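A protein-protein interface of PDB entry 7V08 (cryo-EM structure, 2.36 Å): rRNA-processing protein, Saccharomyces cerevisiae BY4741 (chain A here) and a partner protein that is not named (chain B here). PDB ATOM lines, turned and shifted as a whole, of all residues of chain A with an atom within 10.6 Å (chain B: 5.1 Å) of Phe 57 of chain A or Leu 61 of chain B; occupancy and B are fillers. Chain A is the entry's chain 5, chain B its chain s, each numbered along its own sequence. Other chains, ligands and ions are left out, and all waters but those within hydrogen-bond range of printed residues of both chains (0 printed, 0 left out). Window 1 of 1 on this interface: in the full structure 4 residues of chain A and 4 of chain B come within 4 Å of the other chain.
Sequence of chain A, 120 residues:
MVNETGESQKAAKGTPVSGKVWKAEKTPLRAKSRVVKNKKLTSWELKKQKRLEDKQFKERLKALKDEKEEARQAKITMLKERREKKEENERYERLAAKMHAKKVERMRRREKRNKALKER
Among the printed residues, merely in contact across the chains: Phe 57 of chain A with Lys 57 of chain B (3.4 Å), Leu 64 of chain A with Glu 65 of chain B (3.5 Å), Phe 57 of chain A with Leu 61 of chain B (3.6 Å), Leu 61 of chain A with Leu 61 of chain B (3.7 Å) and Phe 57 of chain A with Ile 50 of chain B (3.9 Å).
The side-chain carboxylate (OD1) of Asp 54 of chain A is in salt-bridge range of the side-chain amino group (NZ) of Lys 57 of chain B (2.9 Å).
Of the printed residues of chain B, Phe 57 of chain A touches Ile 50 (3.9 Å), Lys 57 (3.4 Å) and Leu 61 (3.6 Å). Leu 61 of chain B touches just these residues of chain A: Phe 57 (3.6 Å) and Leu 61 (3.7 Å). Of chain A, only Asp 54 and Phe 57 come within 4 Å of Lys 57 of chain B. No residue of chain A comes within 4 Å of Ala 58 of chain B. No residue of chain A comes within 4 Å of Ile 60 of chain B. No residue of chain A comes within 4 Å of Ile 64 of chain B. Of the printed residues of chain B, Leu 64 of chain A touches Glu 65. Of the printed residues of chain B, Asp 54 of chain A touches Lys 57. Printed residues of chain B within 4 Å of Leu 61 of chain A: Leu 61 (3.7 Å). Asp 66 of chain A touches none of the printed residues of chain B. Lys 58 of chain A touches none of the printed residues of chain B. The nearest residue of chain B that does not touch Phe 57 of chain A is Ala 58 of chain B (4.3 Å). The nearest residue of chain A that does not touch Leu 61 of chain B is Leu 64 of chain A (4.05 Å). The nearest printed residue of chain B that does not touch Asp 54 of chain A is Ala 58 of chain B (8.5 Å).
Printed residues of chain A that touch a printed residue of chain B: Asp 54, Phe 57, Leu 61 and Leu 64. Hydrophobic or aromatic side chains of chain A that line the printed part of chain B: Phe 57, Leu 61 and Leu 64. Of the 11 printed residues of chain B, 4 touch a printed residue of chain A. Hydrophobic or aromatic side chains of chain B that line the printed part of chain A: Ile 50 and Leu 61. Among the printed residues, 6 pairs touch across the chains.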
ATOM      1  N   GLN A  49      -8.213  -9.797 -28.242  1.00  0.00           N
ATOM      2  CA  GLN A  49      -7.935  -8.521 -27.587  1.00  0.00           C
ATOM      3  C   GLN A  49      -9.207  -7.893 -27.029  1.00  0.00           C
ATOM      4  O   GLN A  49      -9.200  -7.322 -25.929  1.00  0.00           O
ATOM      5  CB  GLN A  49      -7.245  -7.574 -28.569  1.00  0.00           C
ATOM      6  CG  GLN A  49      -6.996  -6.164 -28.034  1.00  0.00           C
ATOM      7  CD  GLN A  49      -5.877  -6.095 -27.003  1.00  0.00           C
ATOM      8  OE1 GLN A  49      -5.287  -7.108 -26.627  1.00  0.00           O
ATOM      9  NE2 GLN A  49      -5.576  -4.884 -26.548  1.00  0.00           N
ATOM     10  N   LYS A  50     -10.311  -7.992 -27.772  1.00  0.00           N
ATOM     11  CA  LYS A  50     -11.584  -7.477 -27.284  1.00  0.00           C
ATOM     12  C   LYS A  50     -12.047  -8.230 -26.043  1.00  0.00           C
ATOM     13  O   LYS A  50     -12.581  -7.624 -25.106  1.00  0.00           O
ATOM     14  CB  LYS A  50     -12.636  -7.546 -28.392  1.00  0.00           C
ATOM     15  CG  LYS A  50     -12.457  -6.488 -29.473  1.00  0.00           C
ATOM     16  CD  LYS A  50     -12.678  -5.090 -28.920  1.00  0.00           C
ATOM     17  CE  LYS A  50     -12.372  -4.025 -29.963  1.00  0.00           C
ATOM     18  NZ  LYS A  50     -10.919  -3.970 -30.315  1.00  0.00           N
ATOM     19  N   ARG A  51     -11.847  -9.551 -26.015  1.00  0.00           N
ATOM     20  CA  ARG A  51     -12.183 -10.321 -24.819  1.00  0.00           C
ATOM     21  C   ARG A  51     -11.341  -9.891 -23.621  1.00  0.00           C
ATOM     22  O   ARG A  51     -11.854  -9.768 -22.499  1.00  0.00           O
ATOM     23  CB  ARG A  51     -12.003 -11.815 -25.083  1.00  0.00           C
ATOM     24  CG  ARG A  51     -12.966 -12.384 -26.101  1.00  0.00           C
ATOM     25  CD  ARG A  51     -12.703 -13.853 -26.333  1.00  0.00           C
ATOM     26  NE  ARG A  51     -11.338 -14.099 -26.777  1.00  0.00           N
ATOM     27  CZ  ARG A  51     -10.783 -15.298 -26.868  1.00  0.00           C
ATOM     28  NH1 ARG A  51     -11.449 -16.395 -26.548  1.00  0.00           N
ATOM     29  NH2 ARG A  51      -9.526 -15.399 -27.286  1.00  0.00           N
ATOM     30  N   LEU A  52     -10.043  -9.659 -23.842  1.00  0.00           N
ATOM     31  CA  LEU A  52      -9.177  -9.211 -22.756  1.00  0.00           C
ATOM     32  C   LEU A  52      -9.620  -7.854 -22.213  1.00  0.00           C
ATOM     33  O   LEU A  52      -9.671  -7.650 -20.993  1.00  0.00           O
ATOM     34  CB  LEU A  52      -7.727  -9.150 -23.234  1.00  0.00           C
ATOM     35  CG  LEU A  52      -6.725  -8.686 -22.177  1.00  0.00           C
ATOM     36  CD1 LEU A  52      -6.668  -9.670 -21.010  1.00  0.00           C
ATOM     37  CD2 LEU A  52      -5.343  -8.471 -22.778  1.00  0.00           C
ATOM     38  N   GLU A  53      -9.954  -6.917 -23.107  1.00  0.00           N
ATOM     39  CA  GLU A  53     -10.429  -5.608 -22.662  1.00  0.00           C
ATOM     40  C   GLU A  53     -11.758  -5.718 -21.922  1.00  0.00           C
ATOM     41  O   GLU A  53     -11.987  -5.002 -20.939  1.00  0.00           O
ATOM     42  CB  GLU A  53     -10.553  -4.652 -23.845  1.00  0.00           C
ATOM     43  CG  GLU A  53      -9.237  -4.002 -24.251  1.00  0.00           C
ATOM     44  CD  GLU A  53      -9.392  -3.035 -25.415  1.00  0.00           C
ATOM     45  OE1 GLU A  53     -10.544  -2.736 -25.800  1.00  0.00           O
ATOM     46  OE2 GLU A  53      -8.361  -2.578 -25.951  1.00  0.00           O
ATOM     47  N   ASP A  54     -12.646  -6.602 -22.383  1.00  0.00           N
ATOM     48  CA  ASP A  54     -13.919  -6.792 -21.696  1.00  0.00           C
ATOM     49  C   ASP A  54     -13.709  -7.301 -20.275  1.00  0.00           C
ATOM     50  O   ASP A  54     -14.351  -6.821 -19.331  1.00  0.00           O
ATOM     51  CB  ASP A  54     -14.797  -7.753 -22.495  1.00  0.00           C
ATOM     52  CG  ASP A  54     -16.250  -7.708 -22.071  1.00  0.00           C
ATOM     53  OD1 ASP A  54     -16.886  -6.650 -22.248  1.00  0.00           O
ATOM     54  OD2 ASP A  54     -16.757  -8.734 -21.572  1.00  0.00           O
ATOM     55  N   LYS A  55     -12.797  -8.265 -20.098  1.00  0.00           N
ATOM     56  CA  LYS A  55     -12.510  -8.762 -18.753  1.00  0.00           C
ATOM     57  C   LYS A  55     -11.885  -7.682 -17.875  1.00  0.00           C
ATOM     58  O   LYS A  55     -12.202  -7.582 -16.683  1.00  0.00           O
ATOM     59  CB  LYS A  55     -11.597  -9.984 -18.818  1.00  0.00           C
ATOM     60  CG  LYS A  55     -12.310 -11.245 -19.230  1.00  0.00           C
ATOM     61  CD  LYS A  55     -11.504 -12.472 -18.874  1.00  0.00           C
ATOM     62  CE  LYS A  55     -11.974 -13.662 -19.680  1.00  0.00           C
ATOM     63  NZ  LYS A  55     -12.004 -13.337 -21.133  1.00  0.00           N
ATOM     64  N   GLN A  56     -10.980  -6.877 -18.439  1.00  0.00           N
ATOM     65  CA  GLN A  56     -10.372  -5.803 -17.658  1.00  0.00           C
ATOM     66  C   GLN A  56     -11.405  -4.766 -17.220  1.00  0.00           C
ATOM     67  O   GLN A  56     -11.384  -4.303 -16.070  1.00  0.00           O
ATOM     68  CB  GLN A  56      -9.247  -5.150 -18.456  1.00  0.00           C
ATOM     69  CG  GLN A  56      -8.004  -6.011 -18.555  1.00  0.00           C
ATOM     70  CD  GLN A  56      -6.910  -5.356 -19.374  1.00  0.00           C
ATOM     71  OE1 GLN A  56      -7.182  -4.515 -20.227  1.00  0.00           O
ATOM     72  NE2 GLN A  56      -5.667  -5.739 -19.115  1.00  0.00           N
ATOM     73  N   PHE A  57     -12.329  -4.400 -18.116  1.00  0.00           N
ATOM     74  CA  PHE A  57     -13.395  -3.485 -17.722  1.00  0.00           C
ATOM     75  C   PHE A  57     -14.266  -4.091 -16.630  1.00  0.00           C
ATOM     76  O   PHE A  57     -14.669  -3.393 -15.690  1.00  0.00           O
ATOM     77  CB  PHE A  57     -14.263  -3.104 -18.923  1.00  0.00           C
ATOM     78  CG  PHE A  57     -15.500  -2.320 -18.545  1.00  0.00           C
ATOM     79  CD1 PHE A  57     -15.438  -0.948 -18.381  1.00  0.00           C
ATOM     80  CD2 PHE A  57     -16.718  -2.956 -18.347  1.00  0.00           C
ATOM     81  CE1 PHE A  57     -16.560  -0.225 -18.025  1.00  0.00           C
ATOM     82  CE2 PHE A  57     -17.843  -2.234 -17.984  1.00  0.00           C
ATOM     83  CZ  PHE A  57     -17.764  -0.868 -17.829  1.00  0.00           C
ATOM     84  N   LYS A  58     -14.600  -5.379 -16.759  1.00  0.00           N
ATOM     85  CA  LYS A  58     -15.457  -6.013 -15.763  1.00  0.00           C
ATOM     86  C   LYS A  58     -14.778  -6.056 -14.402  1.00  0.00           C
ATOM     87  O   LYS A  58     -15.426  -5.838 -13.374  1.00  0.00           O
ATOM     88  CB  LYS A  58     -15.861  -7.415 -16.222  1.00  0.00           C
ATOM     89  CG  LYS A  58     -16.981  -7.414 -17.253  1.00  0.00           C
ATOM     90  CD  LYS A  58     -17.454  -8.817 -17.583  1.00  0.00           C
ATOM     91  CE  LYS A  58     -18.214  -9.443 -16.417  1.00  0.00           C
ATOM     92  NZ  LYS A  58     -19.562  -8.835 -16.216  1.00  0.00           N
ATOM     93  N   GLU A  59     -13.467  -6.305 -14.373  1.00  0.00           N
ATOM     94  CA  GLU A  59     -12.776  -6.326 -13.089  1.00  0.00           C
ATOM     95  C   GLU A  59     -12.662  -4.925 -12.489  1.00  0.00           C
ATOM     96  O   GLU A  59     -12.772  -4.766 -11.266  1.00  0.00           O
ATOM     97  CB  GLU A  59     -11.406  -6.997 -13.223  1.00  0.00           C
ATOM     98  CG  GLU A  59     -10.263  -6.108 -13.658  1.00  0.00           C
ATOM     99  CD  GLU A  59      -8.922  -6.789 -13.532  1.00  0.00           C
ATOM    100  OE1 GLU A  59      -8.874  -7.906 -12.976  1.00  0.00           O
ATOM    101  OE2 GLU A  59      -7.919  -6.210 -13.992  1.00  0.00           O
ATOM    102  N   ARG A  60     -12.480  -3.889 -13.321  1.00  0.00           N
ATOM    103  CA  ARG A  60     -12.458  -2.528 -12.782  1.00  0.00           C
ATOM    104  C   ARG A  60     -13.811  -2.148 -12.188  1.00  0.00           C
ATOM    105  O   ARG A  60     -13.883  -1.580 -11.086  1.00  0.00           O
ATOM    106  CB  ARG A  60     -12.058  -1.526 -13.864  1.00  0.00           C
ATOM    107  CG  ARG A  60     -10.602  -1.593 -14.281  1.00  0.00           C
ATOM    108  CD  ARG A  60      -9.669  -1.515 -13.081  1.00  0.00           C
ATOM    109  NE  ARG A  60      -9.803  -0.268 -12.338  1.00  0.00           N
ATOM    110  CZ  ARG A  60      -9.162  -0.003 -11.208  1.00  0.00           C
ATOM    111  NH1 ARG A  60      -8.321  -0.872 -10.671  1.00  0.00           N
ATOM    112  NH2 ARG A  60      -9.380   1.157 -10.595  1.00  0.00           N
ATOM    113  N   LEU A  61     -14.894  -2.466 -12.901  1.00  0.00           N
ATOM    114  CA  LEU A  61     -16.226  -2.159 -12.395  1.00  0.00           C
ATOM    115  C   LEU A  61     -16.527  -2.949 -11.127  1.00  0.00           C
ATOM    116  O   LEU A  61     -17.132  -2.421 -10.186  1.00  0.00           O
ATOM    117  CB  LEU A  61     -17.275  -2.444 -13.472  1.00  0.00           C
ATOM    118  CG  LEU A  61     -18.651  -1.836 -13.205  1.00  0.00           C
ATOM    119  CD1 LEU A  61     -18.545  -0.321 -13.166  1.00  0.00           C
ATOM    120  CD2 LEU A  61     -19.671  -2.274 -14.240  1.00  0.00           C
ATOM    121  N   LYS A  62     -16.104  -4.213 -11.082  1.00  0.00           N
ATOM    122  CA  LYS A  62     -16.303  -5.022  -9.886  1.00  0.00           C
ATOM    123  C   LYS A  62     -15.544  -4.447  -8.697  1.00  0.00           C
ATOM    124  O   LYS A  62     -16.068  -4.419  -7.580  1.00  0.00           O
ATOM    125  CB  LYS A  62     -15.867  -6.461 -10.154  1.00  0.00           C
ATOM    126  CG  LYS A  62     -15.990  -7.391  -8.957  1.00  0.00           C
ATOM    127  CD  LYS A  62     -15.554  -8.799  -9.315  1.00  0.00           C
ATOM    128  CE  LYS A  62     -15.502  -9.697  -8.093  1.00  0.00           C
ATOM    129  NZ  LYS A  62     -14.538  -9.192  -7.085  1.00  0.00           N
ATOM    130  N   ALA A  63     -14.307  -3.988  -8.917  1.00  0.00           N
ATOM    131  CA  ALA A  63     -13.530  -3.410  -7.824  1.00  0.00           C
ATOM    132  C   ALA A  63     -14.185  -2.140  -7.291  1.00  0.00           C
ATOM    133  O   ALA A  63     -14.269  -1.941  -6.072  1.00  0.00           O
ATOM    134  CB  ALA A  63     -12.101  -3.127  -8.286  1.00  0.00           C
ATOM    135  N   LEU A  64     -14.661  -1.276  -8.194  1.00  0.00           N
ATOM    136  CA  LEU A  64     -15.344  -0.061  -7.757  1.00  0.00           C
ATOM    137  C   LEU A  64     -16.620  -0.384  -6.985  1.00  0.00           C
ATOM    138  O   LEU A  64     -16.887   0.209  -5.929  1.00  0.00           O
ATOM    139  CB  LEU A  64     -15.641   0.827  -8.964  1.00  0.00           C
ATOM    140  CG  LEU A  64     -14.389   1.407  -9.625  1.00  0.00           C
ATOM    141  CD1 LEU A  64     -14.644   1.759 -11.081  1.00  0.00           C
ATOM    142  CD2 LEU A  64     -13.882   2.621  -8.854  1.00  0.00           C
ATOM    143  N   LYS A  65     -17.410  -1.341  -7.481  1.00  0.00           N
ATOM    144  CA  LYS A  65     -18.633  -1.723  -6.783  1.00  0.00           C
ATOM    145  C   LYS A  65     -18.328  -2.324  -5.416  1.00  0.00           C
ATOM    146  O   LYS A  65     -19.026  -2.039  -4.436  1.00  0.00           O
ATOM    147  CB  LYS A  65     -19.437  -2.707  -7.635  1.00  0.00           C
ATOM    148  CG  LYS A  65     -20.022  -2.084  -8.887  1.00  0.00           C
ATOM    149  CD  LYS A  65     -20.786  -3.093  -9.716  1.00  0.00           C
ATOM    150  CE  LYS A  65     -21.624  -2.387 -10.763  1.00  0.00           C
ATOM    151  NZ  LYS A  65     -22.554  -1.413 -10.119  1.00  0.00           N
ATOM    152  N   ASP A  66     -17.286  -3.157  -5.335  1.00  0.00           N
ATOM    153  CA  ASP A  66     -16.924  -3.786  -4.071  1.00  0.00           C
ATOM    154  C   ASP A  66     -16.457  -2.760  -3.048  1.00  0.00           C
ATOM    155  O   ASP A  66     -16.819  -2.855  -1.871  1.00  0.00           O
ATOM    156  CB  ASP A  66     -15.846  -4.843  -4.300  1.00  0.00           C
ATOM    157  CG  ASP A  66     -16.388  -6.086  -4.969  1.00  0.00           C
ATOM    158  OD1 ASP A  66     -17.556  -6.441  -4.704  1.00  0.00           O
ATOM    159  OD2 ASP A  66     -15.648  -6.702  -5.764  1.00  0.00           O
ATOM    160  N   GLU A  67     -15.659  -1.772  -3.466  1.00  0.00           N
ATOM    161  CA  GLU A  67     -15.219  -0.773  -2.495  1.00  0.00           C
ATOM    162  C   GLU A  67     -16.381   0.113  -2.050  1.00  0.00           C
ATOM    163  O   GLU A  67     -16.476   0.464  -0.864  1.00  0.00           O
ATOM    164  CB  GLU A  67     -14.050   0.057  -3.041  1.00  0.00           C
ATOM    165  CG  GLU A  67     -14.300   0.846  -4.313  1.00  0.00           C
ATOM    166  CD  GLU A  67     -14.954   2.193  -4.065  1.00  0.00           C
ATOM    167  OE1 GLU A  67     -14.650   2.830  -3.035  1.00  0.00           O
ATOM    168  OE2 GLU A  67     -15.787   2.610  -4.899  1.00  0.00           O
ATOM    169  N   ILE B  50     -23.896   0.783 -17.048  1.00  0.00           N
ATOM    170  CA  ILE B  50     -23.457   0.824 -18.445  1.00  0.00           C
ATOM    171  C   ILE B  50     -23.799  -0.504 -19.111  1.00  0.00           C
ATOM    172  O   ILE B  50     -23.527  -1.566 -18.529  1.00  0.00           O
ATOM    173  CB  ILE B  50     -21.963   1.106 -18.526  1.00  0.00           C
ATOM    174  CG1 ILE B  50     -21.533   2.060 -17.411  1.00  0.00           C
ATOM    175  CG2 ILE B  50     -21.620   1.694 -19.879  1.00  0.00           C
ATOM    176  CD1 ILE B  50     -20.033   2.215 -17.292  1.00  0.00           C
ATOM    177  N   LYS B  57     -17.381   1.942 -23.101  1.00  0.00           N
ATOM    178  CA  LYS B  57     -17.520   1.676 -21.672  1.00  0.00           C
ATOM    179  C   LYS B  57     -16.313   2.179 -20.901  1.00  0.00           C
ATOM    180  O   LYS B  57     -16.452   2.727 -19.801  1.00  0.00           O
ATOM    181  CB  LYS B  57     -17.686   0.176 -21.425  1.00  0.00           C
ATOM    182  CG  LYS B  57     -19.075  -0.370 -21.592  1.00  0.00           C
ATOM    183  CD  LYS B  57     -19.105  -1.856 -21.285  1.00  0.00           C
ATOM    184  CE  LYS B  57     -18.059  -2.615 -22.089  1.00  0.00           C
ATOM    185  NZ  LYS B  57     -18.097  -4.076 -21.815  1.00  0.00           N
ATOM    186  N   ALA B  58     -15.116   1.971 -21.455  1.00  0.00           N
ATOM    187  CA  ALA B  58     -13.891   2.375 -20.777  1.00  0.00           C
ATOM    188  C   ALA B  58     -13.814   3.882 -20.625  1.00  0.00           C
ATOM    189  O   ALA B  58     -13.422   4.383 -19.568  1.00  0.00           O
ATOM    190  CB  ALA B  58     -12.674   1.850 -21.535  1.00  0.00           C
ATOM    191  N   LYS B  59     -14.180   4.625 -21.675  1.00  0.00           N
ATOM    192  CA  LYS B  59     -14.200   6.080 -21.580  1.00  0.00           C
ATOM    193  C   LYS B  59     -15.226   6.549 -20.559  1.00  0.00           C
ATOM    194  O   LYS B  59     -14.953   7.471 -19.780  1.00  0.00           O
ATOM    195  CB  LYS B  59     -14.489   6.700 -22.947  1.00  0.00           C
ATOM    196  CG  LYS B  59     -13.442   6.420 -24.006  1.00  0.00           C
ATOM    197  CD  LYS B  59     -13.961   6.786 -25.390  1.00  0.00           C
ATOM    198  CE  LYS B  59     -12.982   6.350 -26.470  1.00  0.00           C
ATOM    199  NZ  LYS B  59     -12.626   4.909 -26.314  1.00  0.00           N
ATOM    200  N   ILE B  60     -16.410   5.922 -20.540  1.00  0.00           N
ATOM    201  CA  ILE B  60     -17.426   6.309 -19.561  1.00  0.00           C
ATOM    202  C   ILE B  60     -16.929   6.070 -18.137  1.00  0.00           C
ATOM    203  O   ILE B  60     -17.090   6.925 -17.253  1.00  0.00           O
ATOM    204  CB  ILE B  60     -18.746   5.563 -19.833  1.00  0.00           C
ATOM    205  CG1 ILE B  60     -19.403   6.091 -21.105  1.00  0.00           C
ATOM    206  CG2 ILE B  60     -19.696   5.688 -18.646  1.00  0.00           C
ATOM    207  CD1 ILE B  60     -19.845   7.534 -21.006  1.00  0.00           C
ATOM    208  N   LEU B  61     -16.300   4.919 -17.898  1.00  0.00           N
ATOM    209  CA  LEU B  61     -15.805   4.618 -16.558  1.00  0.00           C
ATOM    210  C   LEU B  61     -14.659   5.542 -16.162  1.00  0.00           C
ATOM    211  O   LEU B  61     -14.600   6.006 -15.020  1.00  0.00           O
ATOM    212  CB  LEU B  61     -15.370   3.156 -16.467  1.00  0.00           C
ATOM    213  CG  LEU B  61     -15.462   2.558 -15.063  1.00  0.00           C
ATOM    214  CD1 LEU B  61     -16.886   2.696 -14.532  1.00  0.00           C
ATOM    215  CD2 LEU B  61     -15.031   1.103 -15.055  1.00  0.00           C
ATOM    216  N   GLU B  62     -13.739   5.820 -17.090  1.00  0.00           N
ATOM    217  CA  GLU B  62     -12.631   6.719 -16.787  1.00  0.00           C
ATOM    218  C   GLU B  62     -13.132   8.117 -16.464  1.00  0.00           C
ATOM    219  O   GLU B  62     -12.636   8.764 -15.532  1.00  0.00           O
ATOM    220  CB  GLU B  62     -11.652   6.764 -17.958  1.00  0.00           C
ATOM    221  CG  GLU B  62     -10.640   5.639 -17.968  1.00  0.00           C
ATOM    222  CD  GLU B  62      -9.930   5.509 -19.298  1.00  0.00           C
ATOM    223  OE1 GLU B  62     -10.431   6.069 -20.298  1.00  0.00           O
ATOM    224  OE2 GLU B  62      -8.872   4.846 -19.347  1.00  0.00           O
ATOM    225  N   GLU B  63     -14.119   8.600 -17.221  1.00  0.00           N
ATOM    226  CA  GLU B  63     -14.681   9.914 -16.944  1.00  0.00           C
ATOM    227  C   GLU B  63     -15.389   9.941 -15.598  1.00  0.00           C
ATOM    228  O   GLU B  63     -15.273  10.919 -14.859  1.00  0.00           O
ATOM    229  CB  GLU B  63     -15.627  10.337 -18.065  1.00  0.00           C
ATOM    230  CG  GLU B  63     -14.903  10.655 -19.361  1.00  0.00           C
ATOM    231  CD  GLU B  63     -15.732  11.502 -20.305  1.00  0.00           C
ATOM    232  OE1 GLU B  63     -16.709  12.125 -19.838  1.00  0.00           O
ATOM    233  OE2 GLU B  63     -15.401  11.539 -21.513  1.00  0.00           O
ATOM    234  N   ILE B  64     -16.112   8.872 -15.250  1.00  0.00           N
ATOM    235  CA  ILE B  64     -16.802   8.888 -13.959  1.00  0.00           C
ATOM    236  C   ILE B  64     -15.800   8.812 -12.802  1.00  0.00           C
ATOM    237  O   ILE B  64     -16.001   9.448 -11.758  1.00  0.00           O
ATOM    238  CB  ILE B  64     -17.884   7.785 -13.904  1.00  0.00           C
ATOM    239  CG1 ILE B  64     -19.084   8.263 -13.083  1.00  0.00           C
ATOM    240  CG2 ILE B  64     -17.365   6.478 -13.323  1.00  0.00           C
ATOM    241  CD1 ILE B  64     -19.797   9.470 -13.669  1.00  0.00           C
ATOM    242  N   GLU B  65     -14.679   8.104 -12.981  1.00  0.00           N
ATOM    243  CA  GLU B  65     -13.662   8.062 -11.930  1.00  0.00           C
ATOM    244  C   GLU B  65     -12.954   9.405 -11.783  1.00  0.00           C
ATOM    245  O   GLU B  65     -12.679   9.851 -10.660  1.00  0.00           O
ATOM    246  CB  GLU B  65     -12.642   6.962 -12.217  1.00  0.00           C
ATOM    247  CG  GLU B  65     -13.208   5.558 -12.233  1.00  0.00           C
ATOM    248  CD  GLU B  65     -12.165   4.529 -12.606  1.00  0.00           C
ATOM    249  OE1 GLU B  65     -10.984   4.729 -12.255  1.00  0.00           O
ATOM    250  OE2 GLU B  65     -12.523   3.521 -13.254  1.00  0.00           O
ATOM    251  N   ALA B  66     -12.636  10.058 -12.903  1.00  0.00           N
ATOM    252  CA  ALA B  66     -12.008  11.374 -12.831  1.00  0.00           C
ATOM    253  C   ALA B  66     -12.960  12.404 -12.234  1.00  0.00           C
ATOM    254  O   ALA B  66     -12.538  13.283 -11.473  1.00  0.00           O
ATOM    255  CB  ALA B  66     -11.531  11.805 -14.218  1.00  0.00           C
